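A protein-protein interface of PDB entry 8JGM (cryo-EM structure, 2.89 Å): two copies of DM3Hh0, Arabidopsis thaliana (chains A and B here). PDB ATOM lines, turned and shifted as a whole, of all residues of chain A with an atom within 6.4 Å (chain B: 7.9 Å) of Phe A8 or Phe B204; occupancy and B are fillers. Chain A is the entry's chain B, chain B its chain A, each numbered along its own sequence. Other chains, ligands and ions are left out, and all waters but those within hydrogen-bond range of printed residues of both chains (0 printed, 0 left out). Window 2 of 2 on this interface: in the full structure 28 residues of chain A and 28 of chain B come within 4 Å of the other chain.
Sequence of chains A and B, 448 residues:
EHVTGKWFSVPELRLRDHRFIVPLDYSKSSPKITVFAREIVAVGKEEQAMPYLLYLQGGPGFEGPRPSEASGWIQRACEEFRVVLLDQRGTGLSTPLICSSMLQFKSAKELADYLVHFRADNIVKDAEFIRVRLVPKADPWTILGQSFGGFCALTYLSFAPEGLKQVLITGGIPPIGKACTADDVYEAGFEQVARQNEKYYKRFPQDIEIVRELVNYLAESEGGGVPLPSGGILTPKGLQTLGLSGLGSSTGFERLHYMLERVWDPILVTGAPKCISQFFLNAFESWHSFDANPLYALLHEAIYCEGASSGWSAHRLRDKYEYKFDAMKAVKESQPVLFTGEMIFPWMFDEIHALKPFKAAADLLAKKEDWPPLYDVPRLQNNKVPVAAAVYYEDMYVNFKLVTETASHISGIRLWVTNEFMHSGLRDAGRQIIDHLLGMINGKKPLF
Among the printed residues, merely in contact across the chains: Phe A8 with Phe B204 (3.7 Å), Val A10 with Arg B203 (3.6 Å), Val A10 with Glu B254 (3.8 Å), Leu A15 with Tyr B258 (3.99 Å) and Arg A38 with Tyr B258 (3.6 Å).
Of chain B, only Phe B204 comes within 4 Å of Phe A8.
Printed residues of chain A within 4 Å of Arg B203: Ser A9 (2.6 Å) and Val A10 (3.6 Å).
Of the printed residues of chain B, Leu A15 touches Tyr B258.
Tyr B200 touches none of the printed residues of chain A.
The nearest printed residue of chain B that does not touch Val A10 is Tyr B258 (4.8 Å).
Of the 11 printed residues of chain A, 5 touch a printed residue of chain B.
Hydrophobic or aromatic side chains of chain B within 4 Å of the printed part of chain A: Phe B204 and Tyr B258.
Among the printed residues, Asp or Glu carboxylates within 4 Å of a Lys or Arg side-chain nitrogen of the other chain: Arg A38 with Glu B261 (2.6 Å).
The backbone carbonyl oxygen (O) of Phe A8 sits at hydrogen-bond distance from the backbone NH (N) of Leu A15 (2.9 Å).
The guanidinium group (NH2) of Arg B203 lies within salt-bridge range of the side-chain carboxylate (OE2) of Glu B254.
NH2 of Arg B203 sits at hydrogen-bond distance from O of Ser A9 (2.6 Å).
NH2 of Arg A38 is in salt-bridge range of OE2 of Glu B261 (2.6 Å).
No position is printed for both chains.
Of the 7 pairs that touch across the chains among the printed residues, none has its exchanged pair printed and touching as well.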
ATOM      1  N   LYS A   6       8.552  -5.832 -22.200  1.00  0.00           N
ATOM      2  CA  LYS A   6       8.875  -5.748 -23.632  1.00  0.00           C
ATOM      3  C   LYS A   6       7.798  -4.958 -24.381  1.00  0.00           C
ATOM      4  O   LYS A   6       6.629  -5.016 -24.006  1.00  0.00           O
ATOM      5  CB  LYS A   6       8.974  -7.164 -24.226  1.00  0.00           C
ATOM      6  CG  LYS A   6       9.995  -8.094 -23.545  1.00  0.00           C
ATOM      7  CD  LYS A   6      11.443  -7.585 -23.554  1.00  0.00           C
ATOM      8  CE  LYS A   6      11.985  -7.438 -24.979  1.00  0.00           C
ATOM      9  NZ  LYS A   6      13.407  -7.020 -24.981  1.00  0.00           N
ATOM     10  N   TRP A   7       8.152  -4.279 -25.470  1.00  0.00           N
ATOM     11  CA  TRP A   7       7.162  -3.698 -26.382  1.00  0.00           C
ATOM     12  C   TRP A   7       6.304  -4.781 -27.042  1.00  0.00           C
ATOM     13  O   TRP A   7       6.813  -5.844 -27.385  1.00  0.00           O
ATOM     14  CB  TRP A   7       7.863  -2.882 -27.469  1.00  0.00           C
ATOM     15  CG  TRP A   7       8.476  -1.601 -27.021  1.00  0.00           C
ATOM     16  CD1 TRP A   7       9.786  -1.398 -26.763  1.00  0.00           C
ATOM     17  CD2 TRP A   7       7.821  -0.323 -26.768  1.00  0.00           C
ATOM     18  NE1 TRP A   7       9.980  -0.089 -26.373  1.00  0.00           N
ATOM     19  CE2 TRP A   7       8.800   0.617 -26.352  1.00  0.00           C
ATOM     20  CE3 TRP A   7       6.489   0.134 -26.845  1.00  0.00           C
ATOM     21  CZ2 TRP A   7       8.481   1.939 -26.019  1.00  0.00           C
ATOM     22  CZ3 TRP A   7       6.153   1.457 -26.511  1.00  0.00           C
ATOM     23  CH2 TRP A   7       7.146   2.359 -26.100  1.00  0.00           C
ATOM     24  N   PHE A   8       5.030  -4.496 -27.290  1.00  0.00           N
ATOM     25  CA  PHE A   8       4.162  -5.299 -28.156  1.00  0.00           C
ATOM     26  C   PHE A   8       3.239  -4.407 -28.987  1.00  0.00           C
ATOM     27  O   PHE A   8       3.180  -3.196 -28.777  1.00  0.00           O
ATOM     28  CB  PHE A   8       3.403  -6.362 -27.356  1.00  0.00           C
ATOM     29  CG  PHE A   8       2.261  -5.859 -26.505  1.00  0.00           C
ATOM     30  CD1 PHE A   8       2.488  -5.486 -25.170  1.00  0.00           C
ATOM     31  CD2 PHE A   8       0.960  -5.806 -27.030  1.00  0.00           C
ATOM     32  CE1 PHE A   8       1.419  -5.067 -24.363  1.00  0.00           C
ATOM     33  CE2 PHE A   8      -0.110  -5.382 -26.226  1.00  0.00           C
ATOM     34  CZ  PHE A   8       0.119  -5.017 -24.891  1.00  0.00           C
ATOM     35  N   SER A   9       2.569  -4.974 -29.985  1.00  0.00           N
ATOM     36  CA  SER A   9       1.869  -4.217 -31.024  1.00  0.00           C
ATOM     37  C   SER A   9       0.389  -4.542 -31.145  1.00  0.00           C
ATOM     38  O   SER A   9      -0.077  -5.650 -30.890  1.00  0.00           O
ATOM     39  CB  SER A   9       2.567  -4.413 -32.365  1.00  0.00           C
ATOM     40  OG  SER A   9       2.528  -5.775 -32.738  1.00  0.00           O
ATOM     41  N   VAL A  10      -0.353  -3.539 -31.592  1.00  0.00           N
ATOM     42  CA  VAL A  10      -1.787  -3.509 -31.886  1.00  0.00           C
ATOM     43  C   VAL A  10      -1.926  -2.702 -33.184  1.00  0.00           C
ATOM     44  O   VAL A  10      -1.035  -1.899 -33.450  1.00  0.00           O
ATOM     45  CB  VAL A  10      -2.506  -2.857 -30.690  1.00  0.00           C
ATOM     46  CG1 VAL A  10      -3.954  -2.457 -30.941  1.00  0.00           C
ATOM     47  CG2 VAL A  10      -2.522  -3.815 -29.499  1.00  0.00           C
ATOM     48  N   LEU A  13      -0.359   0.891 -33.415  1.00  0.00           N
ATOM     49  CA  LEU A  13       0.165   1.324 -32.107  1.00  0.00           C
ATOM     50  C   LEU A  13       1.259   0.396 -31.568  1.00  0.00           C
ATOM     51  O   LEU A  13       1.284  -0.798 -31.859  1.00  0.00           O
ATOM     52  CB  LEU A  13      -0.967   1.385 -31.065  1.00  0.00           C
ATOM     53  CG  LEU A  13      -2.028   2.465 -31.297  1.00  0.00           C
ATOM     54  CD1 LEU A  13      -3.158   2.291 -30.285  1.00  0.00           C
ATOM     55  CD2 LEU A  13      -1.469   3.872 -31.131  1.00  0.00           C
ATOM     56  N   ARG A  14       2.051   0.963 -30.655  1.00  0.00           N
ATOM     57  CA  ARG A  14       3.094   0.270 -29.900  1.00  0.00           C
ATOM     58  C   ARG A  14       2.737   0.468 -28.410  1.00  0.00           C
ATOM     59  O   ARG A  14       2.366   1.571 -28.009  1.00  0.00           O
ATOM     60  CB  ARG A  14       4.470   0.857 -30.206  1.00  0.00           C
ATOM     61  CG  ARG A  14       5.028   0.456 -31.562  1.00  0.00           C
ATOM     62  CD  ARG A  14       5.146  -1.055 -31.684  1.00  0.00           C
ATOM     63  NE  ARG A  14       6.472  -1.532 -31.300  1.00  0.00           N
ATOM     64  CZ  ARG A  14       6.922  -2.759 -31.541  1.00  0.00           C
ATOM     65  NH1 ARG A  14       8.143  -3.108 -31.156  1.00  0.00           N
ATOM     66  NH2 ARG A  14       6.153  -3.640 -32.167  1.00  0.00           N
ATOM     67  N   LEU A  15       2.836  -0.587 -27.597  1.00  0.00           N
ATOM     68  CA  LEU A  15       2.490  -0.523 -26.179  1.00  0.00           C
ATOM     69  C   LEU A  15       3.557  -1.190 -25.315  1.00  0.00           C
ATOM     70  O   LEU A  15       4.196  -2.148 -25.746  1.00  0.00           O
ATOM     71  CB  LEU A  15       1.136  -1.197 -25.921  1.00  0.00           C
ATOM     72  CG  LEU A  15      -0.059  -0.517 -26.600  1.00  0.00           C
ATOM     73  CD1 LEU A  15      -0.400  -1.142 -27.944  1.00  0.00           C
ATOM     74  CD2 LEU A  15      -1.300  -0.661 -25.729  1.00  0.00           C
ATOM     75  N   ARG A  16       3.706  -0.725 -24.077  1.00  0.00           N
ATOM     76  CA  ARG A  16       4.581  -1.295 -23.044  1.00  0.00           C
ATOM     77  C   ARG A  16       3.973  -1.051 -21.671  1.00  0.00           C
ATOM     78  O   ARG A  16       3.298  -0.045 -21.497  1.00  0.00           O
ATOM     79  CB  ARG A  16       5.950  -0.627 -23.184  1.00  0.00           C
ATOM     80  CG  ARG A  16       6.963  -1.072 -22.127  1.00  0.00           C
ATOM     81  CD  ARG A  16       8.376  -0.594 -22.460  1.00  0.00           C
ATOM     82  NE  ARG A  16       8.498   0.874 -22.410  1.00  0.00           N
ATOM     83  CZ  ARG A  16       9.621   1.553 -22.358  1.00  0.00           C
ATOM     84  NH1 ARG A  16      10.782   0.972 -22.361  1.00  0.00           N
ATOM     85  NH2 ARG A  16       9.608   2.848 -22.289  1.00  0.00           N
ATOM     86  N   ASP A  17       4.218  -1.912 -20.689  1.00  0.00           N
ATOM     87  CA  ASP A  17       3.732  -1.747 -19.314  1.00  0.00           C
ATOM     88  C   ASP A  17       4.860  -1.572 -18.293  1.00  0.00           C
ATOM     89  O   ASP A  17       5.882  -2.249 -18.349  1.00  0.00           O
ATOM     90  CB  ASP A  17       2.828  -2.906 -18.886  1.00  0.00           C
ATOM     91  CG  ASP A  17       3.485  -4.293 -18.919  1.00  0.00           C
ATOM     92  OD1 ASP A  17       4.190  -4.603 -19.901  1.00  0.00           O
ATOM     93  OD2 ASP A  17       3.247  -5.091 -17.980  1.00  0.00           O
ATOM     94  N   ARG A  38       0.445   1.794 -18.558  1.00  0.00           N
ATOM     95  CA  ARG A  38       0.911   1.429 -19.901  1.00  0.00           C
ATOM     96  C   ARG A  38       1.245   2.630 -20.812  1.00  0.00           C
ATOM     97  O   ARG A  38       0.390   3.479 -21.067  1.00  0.00           O
ATOM     98  CB  ARG A  38      -0.110   0.521 -20.590  1.00  0.00           C
ATOM     99  CG  ARG A  38      -0.112  -0.912 -20.081  1.00  0.00           C
ATOM    100  CD  ARG A  38      -0.861  -1.835 -21.029  1.00  0.00           C
ATOM    101  NE  ARG A  38      -2.048  -2.412 -20.405  1.00  0.00           N
ATOM    102  CZ  ARG A  38      -2.318  -3.712 -20.375  1.00  0.00           C
ATOM    103  NH1 ARG A  38      -3.423  -4.148 -19.785  1.00  0.00           N
ATOM    104  NH2 ARG A  38      -1.484  -4.579 -20.934  1.00  0.00           N
ATOM    105  N   GLU B 198      -0.166 -20.962 -33.514  1.00  0.00           N
ATOM    106  CA  GLU B 198       1.235 -20.562 -33.703  1.00  0.00           C
ATOM    107  C   GLU B 198       1.387 -19.055 -33.879  1.00  0.00           C
ATOM    108  O   GLU B 198       2.250 -18.454 -33.245  1.00  0.00           O
ATOM    109  CB  GLU B 198       1.861 -21.283 -34.901  1.00  0.00           C
ATOM    110  CG  GLU B 198       2.073 -22.785 -34.674  1.00  0.00           C
ATOM    111  CD  GLU B 198       2.934 -23.119 -33.442  1.00  0.00           C
ATOM    112  OE1 GLU B 198       3.766 -22.285 -33.023  1.00  0.00           O
ATOM    113  OE2 GLU B 198       2.798 -24.239 -32.904  1.00  0.00           O
ATOM    114  N   LYS B 199       0.532 -18.409 -34.677  1.00  0.00           N
ATOM    115  CA  LYS B 199       0.585 -16.949 -34.833  1.00  0.00           C
ATOM    116  C   LYS B 199       0.316 -16.223 -33.517  1.00  0.00           C
ATOM    117  O   LYS B 199       0.963 -15.219 -33.247  1.00  0.00           O
ATOM    118  CB  LYS B 199      -0.367 -16.475 -35.936  1.00  0.00           C
ATOM    119  CG  LYS B 199       0.140 -16.911 -37.320  1.00  0.00           C
ATOM    120  CD  LYS B 199      -0.681 -16.352 -38.491  1.00  0.00           C
ATOM    121  CE  LYS B 199      -2.100 -16.925 -38.487  1.00  0.00           C
ATOM    122  NZ  LYS B 199      -2.942 -16.398 -39.591  1.00  0.00           N
ATOM    123  N   TYR B 200      -0.568 -16.741 -32.666  1.00  0.00           N
ATOM    124  CA  TYR B 200      -0.819 -16.147 -31.355  1.00  0.00           C
ATOM    125  C   TYR B 200       0.433 -16.161 -30.479  1.00  0.00           C
ATOM    126  O   TYR B 200       0.918 -15.103 -30.090  1.00  0.00           O
ATOM    127  CB  TYR B 200      -1.992 -16.837 -30.664  1.00  0.00           C
ATOM    128  CG  TYR B 200      -2.323 -16.203 -29.335  1.00  0.00           C
ATOM    129  CD1 TYR B 200      -3.152 -15.071 -29.303  1.00  0.00           C
ATOM    130  CD2 TYR B 200      -1.767 -16.699 -28.146  1.00  0.00           C
ATOM    131  CE1 TYR B 200      -3.417 -14.426 -28.084  1.00  0.00           C
ATOM    132  CE2 TYR B 200      -2.025 -16.052 -26.924  1.00  0.00           C
ATOM    133  CZ  TYR B 200      -2.846 -14.913 -26.894  1.00  0.00           C
ATOM    134  OH  TYR B 200      -3.088 -14.272 -25.730  1.00  0.00           O
ATOM    135  N   TYR B 201       1.028 -17.326 -30.211  1.00  0.00           N
ATOM    136  CA  TYR B 201       2.209 -17.376 -29.347  1.00  0.00           C
ATOM    137  C   TYR B 201       3.419 -16.663 -29.952  1.00  0.00           C
ATOM    138  O   TYR B 201       4.180 -16.040 -29.219  1.00  0.00           O
ATOM    139  CB  TYR B 201       2.558 -18.816 -28.985  1.00  0.00           C
ATOM    140  CG  TYR B 201       1.513 -19.501 -28.133  1.00  0.00           C
ATOM    141  CD1 TYR B 201       1.195 -18.985 -26.865  1.00  0.00           C
ATOM    142  CD2 TYR B 201       0.862 -20.651 -28.604  1.00  0.00           C
ATOM    143  CE1 TYR B 201       0.219 -19.611 -26.073  1.00  0.00           C
ATOM    144  CE2 TYR B 201      -0.113 -21.281 -27.815  1.00  0.00           C
ATOM    145  CZ  TYR B 201      -0.439 -20.759 -26.550  1.00  0.00           C
ATOM    146  OH  TYR B 201      -1.381 -21.364 -25.793  1.00  0.00           O
ATOM    147  N   LYS B 202       3.579 -16.656 -31.278  1.00  0.00           N
ATOM    148  CA  LYS B 202       4.627 -15.880 -31.955  1.00  0.00           C
ATOM    149  C   LYS B 202       4.488 -14.376 -31.709  1.00  0.00           C
ATOM    150  O   LYS B 202       5.495 -13.680 -31.629  1.00  0.00           O
ATOM    151  CB  LYS B 202       4.585 -16.219 -33.449  1.00  0.00           C
ATOM    152  CG  LYS B 202       5.733 -15.580 -34.238  1.00  0.00           C
ATOM    153  CD  LYS B 202       5.732 -15.985 -35.716  1.00  0.00           C
ATOM    154  CE  LYS B 202       6.000 -17.482 -35.903  1.00  0.00           C
ATOM    155  NZ  LYS B 202       6.097 -17.850 -37.336  1.00  0.00           N
ATOM    156  N   ARG B 203       3.261 -13.897 -31.529  1.00  0.00           N
ATOM    157  CA  ARG B 203       3.026 -12.480 -31.260  1.00  0.00           C
ATOM    158  C   ARG B 203       3.145 -12.114 -29.771  1.00  0.00           C
ATOM    159  O   ARG B 203       3.608 -11.025 -29.430  1.00  0.00           O
ATOM    160  CB  ARG B 203       1.655 -12.055 -31.794  1.00  0.00           C
ATOM    161  CG  ARG B 203       1.535 -10.568 -32.081  1.00  0.00           C
ATOM    162  CD  ARG B 203       0.168 -10.224 -32.651  1.00  0.00           C
ATOM    163  NE  ARG B 203      -0.210  -8.842 -32.370  1.00  0.00           N
ATOM    164  CZ  ARG B 203      -1.395  -8.317 -32.665  1.00  0.00           C
ATOM    165  NH1 ARG B 203      -2.324  -9.059 -33.253  1.00  0.00           N
ATOM    166  NH2 ARG B 203      -1.653  -7.049 -32.373  1.00  0.00           N
ATOM    167  N   PHE B 204       2.724 -13.024 -28.895  1.00  0.00           N
ATOM    168  CA  PHE B 204       2.767 -12.805 -27.439  1.00  0.00           C
ATOM    169  C   PHE B 204       3.562 -13.901 -26.703  1.00  0.00           C
ATOM    170  O   PHE B 204       2.970 -14.741 -26.023  1.00  0.00           O
ATOM    171  CB  PHE B 204       1.335 -12.700 -26.901  1.00  0.00           C
ATOM    172  CG  PHE B 204       0.508 -11.571 -27.469  1.00  0.00           C
ATOM    173  CD1 PHE B 204       0.587 -10.292 -26.903  1.00  0.00           C
ATOM    174  CD2 PHE B 204      -0.379 -11.808 -28.529  1.00  0.00           C
ATOM    175  CE1 PHE B 204      -0.222  -9.254 -27.387  1.00  0.00           C
ATOM    176  CE2 PHE B 204      -1.181 -10.768 -29.020  1.00  0.00           C
ATOM    177  CZ  PHE B 204      -1.107  -9.490 -28.448  1.00  0.00           C
ATOM    178  N   PRO B 205       4.904 -13.949 -26.817  1.00  0.00           N
ATOM    179  CA  PRO B 205       5.691 -15.100 -26.377  1.00  0.00           C
ATOM    180  C   PRO B 205       5.566 -15.443 -24.891  1.00  0.00           C
ATOM    181  O   PRO B 205       5.671 -16.607 -24.508  1.00  0.00           O
ATOM    182  CB  PRO B 205       7.137 -14.750 -26.722  1.00  0.00           C
ATOM    183  CG  PRO B 205       6.995 -13.795 -27.898  1.00  0.00           C
ATOM    184  CD  PRO B 205       5.746 -13.011 -27.530  1.00  0.00           C
ATOM    185  N   GLN B 206       5.322 -14.450 -24.040  1.00  0.00           N
ATOM    186  CA  GLN B 206       5.228 -14.627 -22.594  1.00  0.00           C
ATOM    187  C   GLN B 206       3.998 -15.431 -22.147  1.00  0.00           C
ATOM    188  O   GLN B 206       3.996 -15.958 -21.037  1.00  0.00           O
ATOM    189  CB  GLN B 206       5.310 -13.260 -21.896  1.00  0.00           C
ATOM    190  CG  GLN B 206       4.147 -12.282 -22.142  1.00  0.00           C
ATOM    191  CD  GLN B 206       4.354 -11.352 -23.339  1.00  0.00           C
ATOM    192  OE1 GLN B 206       4.677 -11.766 -24.443  1.00  0.00           O
ATOM    193  NE2 GLN B 206       4.171 -10.062 -23.180  1.00  0.00           N
ATOM    194  N   ASP B 207       2.962 -15.577 -22.974  1.00  0.00           N
ATOM    195  CA  ASP B 207       1.729 -16.259 -22.559  1.00  0.00           C
ATOM    196  C   ASP B 207       1.886 -17.761 -22.333  1.00  0.00           C
ATOM    197  O   ASP B 207       1.105 -18.338 -21.576  1.00  0.00           O
ATOM    198  CB  ASP B 207       0.609 -16.032 -23.578  1.00  0.00           C
ATOM    199  CG  ASP B 207      -0.053 -14.657 -23.471  1.00  0.00           C
ATOM    200  OD1 ASP B 207       0.365 -13.830 -22.632  1.00  0.00           O
ATOM    201  OD2 ASP B 207      -1.037 -14.442 -24.205  1.00  0.00           O
ATOM    202  N   ILE B 208       2.888 -18.405 -22.941  1.00  0.00           N
ATOM    203  CA  ILE B 208       3.084 -19.860 -22.856  1.00  0.00           C
ATOM    204  C   ILE B 208       3.207 -20.316 -21.398  1.00  0.00           C
ATOM    205  O   ILE B 208       2.639 -21.332 -21.004  1.00  0.00           O
ATOM    206  CB  ILE B 208       4.316 -20.278 -23.685  1.00  0.00           C
ATOM    207  CG1 ILE B 208       4.120 -19.921 -25.173  1.00  0.00           C
ATOM    208  CG2 ILE B 208       4.585 -21.783 -23.526  1.00  0.00           C
ATOM    209  CD1 ILE B 208       5.379 -20.106 -26.024  1.00  0.00           C
ATOM    210  N   GLU B 209       3.895 -19.538 -20.565  1.00  0.00           N
ATOM    211  CA  GLU B 209       4.020 -19.813 -19.135  1.00  0.00           C
ATOM    212  C   GLU B 209       2.685 -19.686 -18.403  1.00  0.00           C
ATOM    213  O   GLU B 209       2.359 -20.508 -17.549  1.00  0.00           O
ATOM    214  CB  GLU B 209       5.014 -18.823 -18.514  1.00  0.00           C
ATOM    215  CG  GLU B 209       6.402 -18.828 -19.168  1.00  0.00           C
ATOM    216  CD  GLU B 209       7.050 -20.216 -19.217  1.00  0.00           C
ATOM    217  OE1 GLU B 209       6.795 -21.047 -18.318  1.00  0.00           O
ATOM    218  OE2 GLU B 209       7.854 -20.469 -20.144  1.00  0.00           O
ATOM    219  N   ILE B 210       1.898 -18.666 -18.747  1.00  0.00           N
ATOM    220  CA  ILE B 210       0.635 -18.362 -18.080  1.00  0.00           C
ATOM    221  C   ILE B 210      -0.349 -19.508 -18.281  1.00  0.00           C
ATOM    222  O   ILE B 210      -0.902 -20.026 -17.313  1.00  0.00           O
ATOM    223  CB  ILE B 210       0.043 -17.036 -18.595  1.00  0.00           C
ATOM    224  CG1 ILE B 210       1.040 -15.861 -18.550  1.00  0.00           C
ATOM    225  CG2 ILE B 210      -1.234 -16.686 -17.822  1.00  0.00           C
ATOM    226  CD1 ILE B 210       1.620 -15.560 -17.168  1.00  0.00           C
ATOM    227  N   GLY B 252      -9.800 -10.565 -31.795  1.00  0.00           N
ATOM    228  CA  GLY B 252      -9.725 -11.633 -30.809  1.00  0.00           C
ATOM    229  C   GLY B 252      -8.381 -11.716 -30.088  1.00  0.00           C
ATOM    230  O   GLY B 252      -8.363 -11.836 -28.867  1.00  0.00           O
ATOM    231  N   PHE B 253      -7.259 -11.585 -30.798  1.00  0.00           N
ATOM    232  CA  PHE B 253      -5.932 -11.742 -30.197  1.00  0.00           C
ATOM    233  C   PHE B 253      -5.699 -10.724 -29.077  1.00  0.00           C
ATOM    234  O   PHE B 253      -5.276 -11.093 -27.985  1.00  0.00           O
ATOM    235  CB  PHE B 253      -4.840 -11.588 -31.260  1.00  0.00           C
ATOM    236  CG  PHE B 253      -4.540 -12.773 -32.160  1.00  0.00           C
ATOM    237  CD1 PHE B 253      -3.227 -12.934 -32.638  1.00  0.00           C
ATOM    238  CD2 PHE B 253      -5.520 -13.709 -32.536  1.00  0.00           C
ATOM    239  CE1 PHE B 253      -2.892 -14.013 -33.465  1.00  0.00           C
ATOM    240  CE2 PHE B 253      -5.188 -14.783 -33.377  1.00  0.00           C
ATOM    241  CZ  PHE B 253      -3.873 -14.941 -33.836  1.00  0.00           C
ATOM    242  N   GLU B 254      -5.995  -9.444 -29.302  1.00  0.00           N
ATOM    243  CA  GLU B 254      -5.786  -8.406 -28.297  1.00  0.00           C
ATOM    244  C   GLU B 254      -6.699  -8.616 -27.087  1.00  0.00           C
ATOM    245  O   GLU B 254      -6.239  -8.570 -25.949  1.00  0.00           O
ATOM    246  CB  GLU B 254      -6.022  -7.017 -28.904  1.00  0.00           C
ATOM    247  CG  GLU B 254      -5.025  -6.633 -30.011  1.00  0.00           C
ATOM    248  CD  GLU B 254      -5.258  -7.290 -31.387  1.00  0.00           C
ATOM    249  OE1 GLU B 254      -6.341  -7.867 -31.628  1.00  0.00           O
ATOM    250  OE2 GLU B 254      -4.325  -7.241 -32.223  1.00  0.00           O
ATOM    251  N   ARG B 255      -7.986  -8.908 -27.313  1.00  0.00           N
ATOM    252  CA  ARG B 255      -8.946  -9.146 -26.229  1.00  0.00           C
ATOM    253  C   ARG B 255      -8.563 -10.357 -25.390  1.00  0.00           C
ATOM    254  O   ARG B 255      -8.632 -10.301 -24.166  1.00  0.00           O
ATOM    255  CB  ARG B 255     -10.349  -9.279 -26.830  1.00  0.00           C
ATOM    256  CG  ARG B 255     -11.414  -9.491 -25.744  1.00  0.00           C
ATOM    257  CD  ARG B 255     -12.854  -9.322 -26.245  1.00  0.00           C
ATOM    258  NE  ARG B 255     -13.183 -10.219 -27.371  1.00  0.00           N
ATOM    259  CZ  ARG B 255     -13.222  -9.895 -28.649  1.00  0.00           C
ATOM    260  NH1 ARG B 255     -12.928  -8.700 -29.063  1.00  0.00           N
ATOM    261  NH2 ARG B 255     -13.552 -10.778 -29.542  1.00  0.00           N
ATOM    262  N   LEU B 256      -8.114 -11.435 -26.022  1.00  0.00           N
ATOM    263  CA  LEU B 256      -7.653 -12.627 -25.328  1.00  0.00           C
ATOM    264  C   LEU B 256      -6.422 -12.335 -24.462  1.00  0.00           C
ATOM    265  O   LEU B 256      -6.397 -12.709 -23.293  1.00  0.00           O
ATOM    266  CB  LEU B 256      -7.389 -13.710 -26.379  1.00  0.00           C
ATOM    267  CG  LEU B 256      -6.828 -15.023 -25.824  1.00  0.00           C
ATOM    268  CD1 LEU B 256      -7.742 -15.621 -24.766  1.00  0.00           C
ATOM    269  CD2 LEU B 256      -6.725 -16.037 -26.958  1.00  0.00           C
ATOM    270  N   HIS B 257      -5.435 -11.604 -24.981  1.00  0.00           N
ATOM    271  CA  HIS B 257      -4.244 -11.274 -24.209  1.00  0.00           C
ATOM    272  C   HIS B 257      -4.580 -10.493 -22.937  1.00  0.00           C
ATOM    273  O   HIS B 257      -4.123 -10.863 -21.859  1.00  0.00           O
ATOM    274  CB  HIS B 257      -3.249 -10.507 -25.077  1.00  0.00           C
ATOM    275  CG  HIS B 257      -2.074  -9.995 -24.290  1.00  0.00           C
ATOM    276  ND1 HIS B 257      -1.950  -8.745 -23.739  1.00  0.00           N
ATOM    277  CD2 HIS B 257      -0.989 -10.722 -23.886  1.00  0.00           C
ATOM    278  CE1 HIS B 257      -0.809  -8.707 -23.035  1.00  0.00           C
ATOM    279  NE2 HIS B 257      -0.185  -9.894 -23.097  1.00  0.00           N
ATOM    280  N   TYR B 258      -5.417  -9.453 -23.014  1.00  0.00           N
ATOM    281  CA  TYR B 258      -5.789  -8.699 -21.819  1.00  0.00           C
ATOM    282  C   TYR B 258      -6.517  -9.544 -20.777  1.00  0.00           C
ATOM    283  O   TYR B 258      -6.354  -9.299 -19.589  1.00  0.00           O
ATOM    284  CB  TYR B 258      -6.664  -7.501 -22.181  1.00  0.00           C
ATOM    285  CG  TYR B 258      -5.990  -6.412 -22.984  1.00  0.00           C
ATOM    286  CD1 TYR B 258      -4.696  -5.968 -22.654  1.00  0.00           C
ATOM    287  CD2 TYR B 258      -6.695  -5.788 -24.024  1.00  0.00           C
ATOM    288  CE1 TYR B 258      -4.104  -4.921 -23.376  1.00  0.00           C
ATOM    289  CE2 TYR B 258      -6.110  -4.734 -24.744  1.00  0.00           C
ATOM    290  CZ  TYR B 258      -4.810  -4.304 -24.422  1.00  0.00           C
ATOM    291  OH  TYR B 258      -4.243  -3.277 -25.094  1.00  0.00           O
ATOM    292  N   GLU B 261      -3.905 -11.547 -18.545  1.00  0.00           N
ATOM    293  CA  GLU B 261      -3.202 -10.786 -17.500  1.00  0.00           C
ATOM    294  C   GLU B 261      -3.840 -10.944 -16.101  1.00  0.00           C
ATOM    295  O   GLU B 261      -3.194 -10.655 -15.099  1.00  0.00           O
ATOM    296  CB  GLU B 261      -3.170  -9.292 -17.847  1.00  0.00           C
ATOM    297  CG  GLU B 261      -2.333  -8.940 -19.086  1.00  0.00           C
ATOM    298  CD  GLU B 261      -2.241  -7.417 -19.317  1.00  0.00           C
ATOM    299  OE1 GLU B 261      -3.161  -6.671 -18.923  1.00  0.00           O
ATOM    300  OE2 GLU B 261      -1.252  -6.931 -19.917  1.00  0.00           O
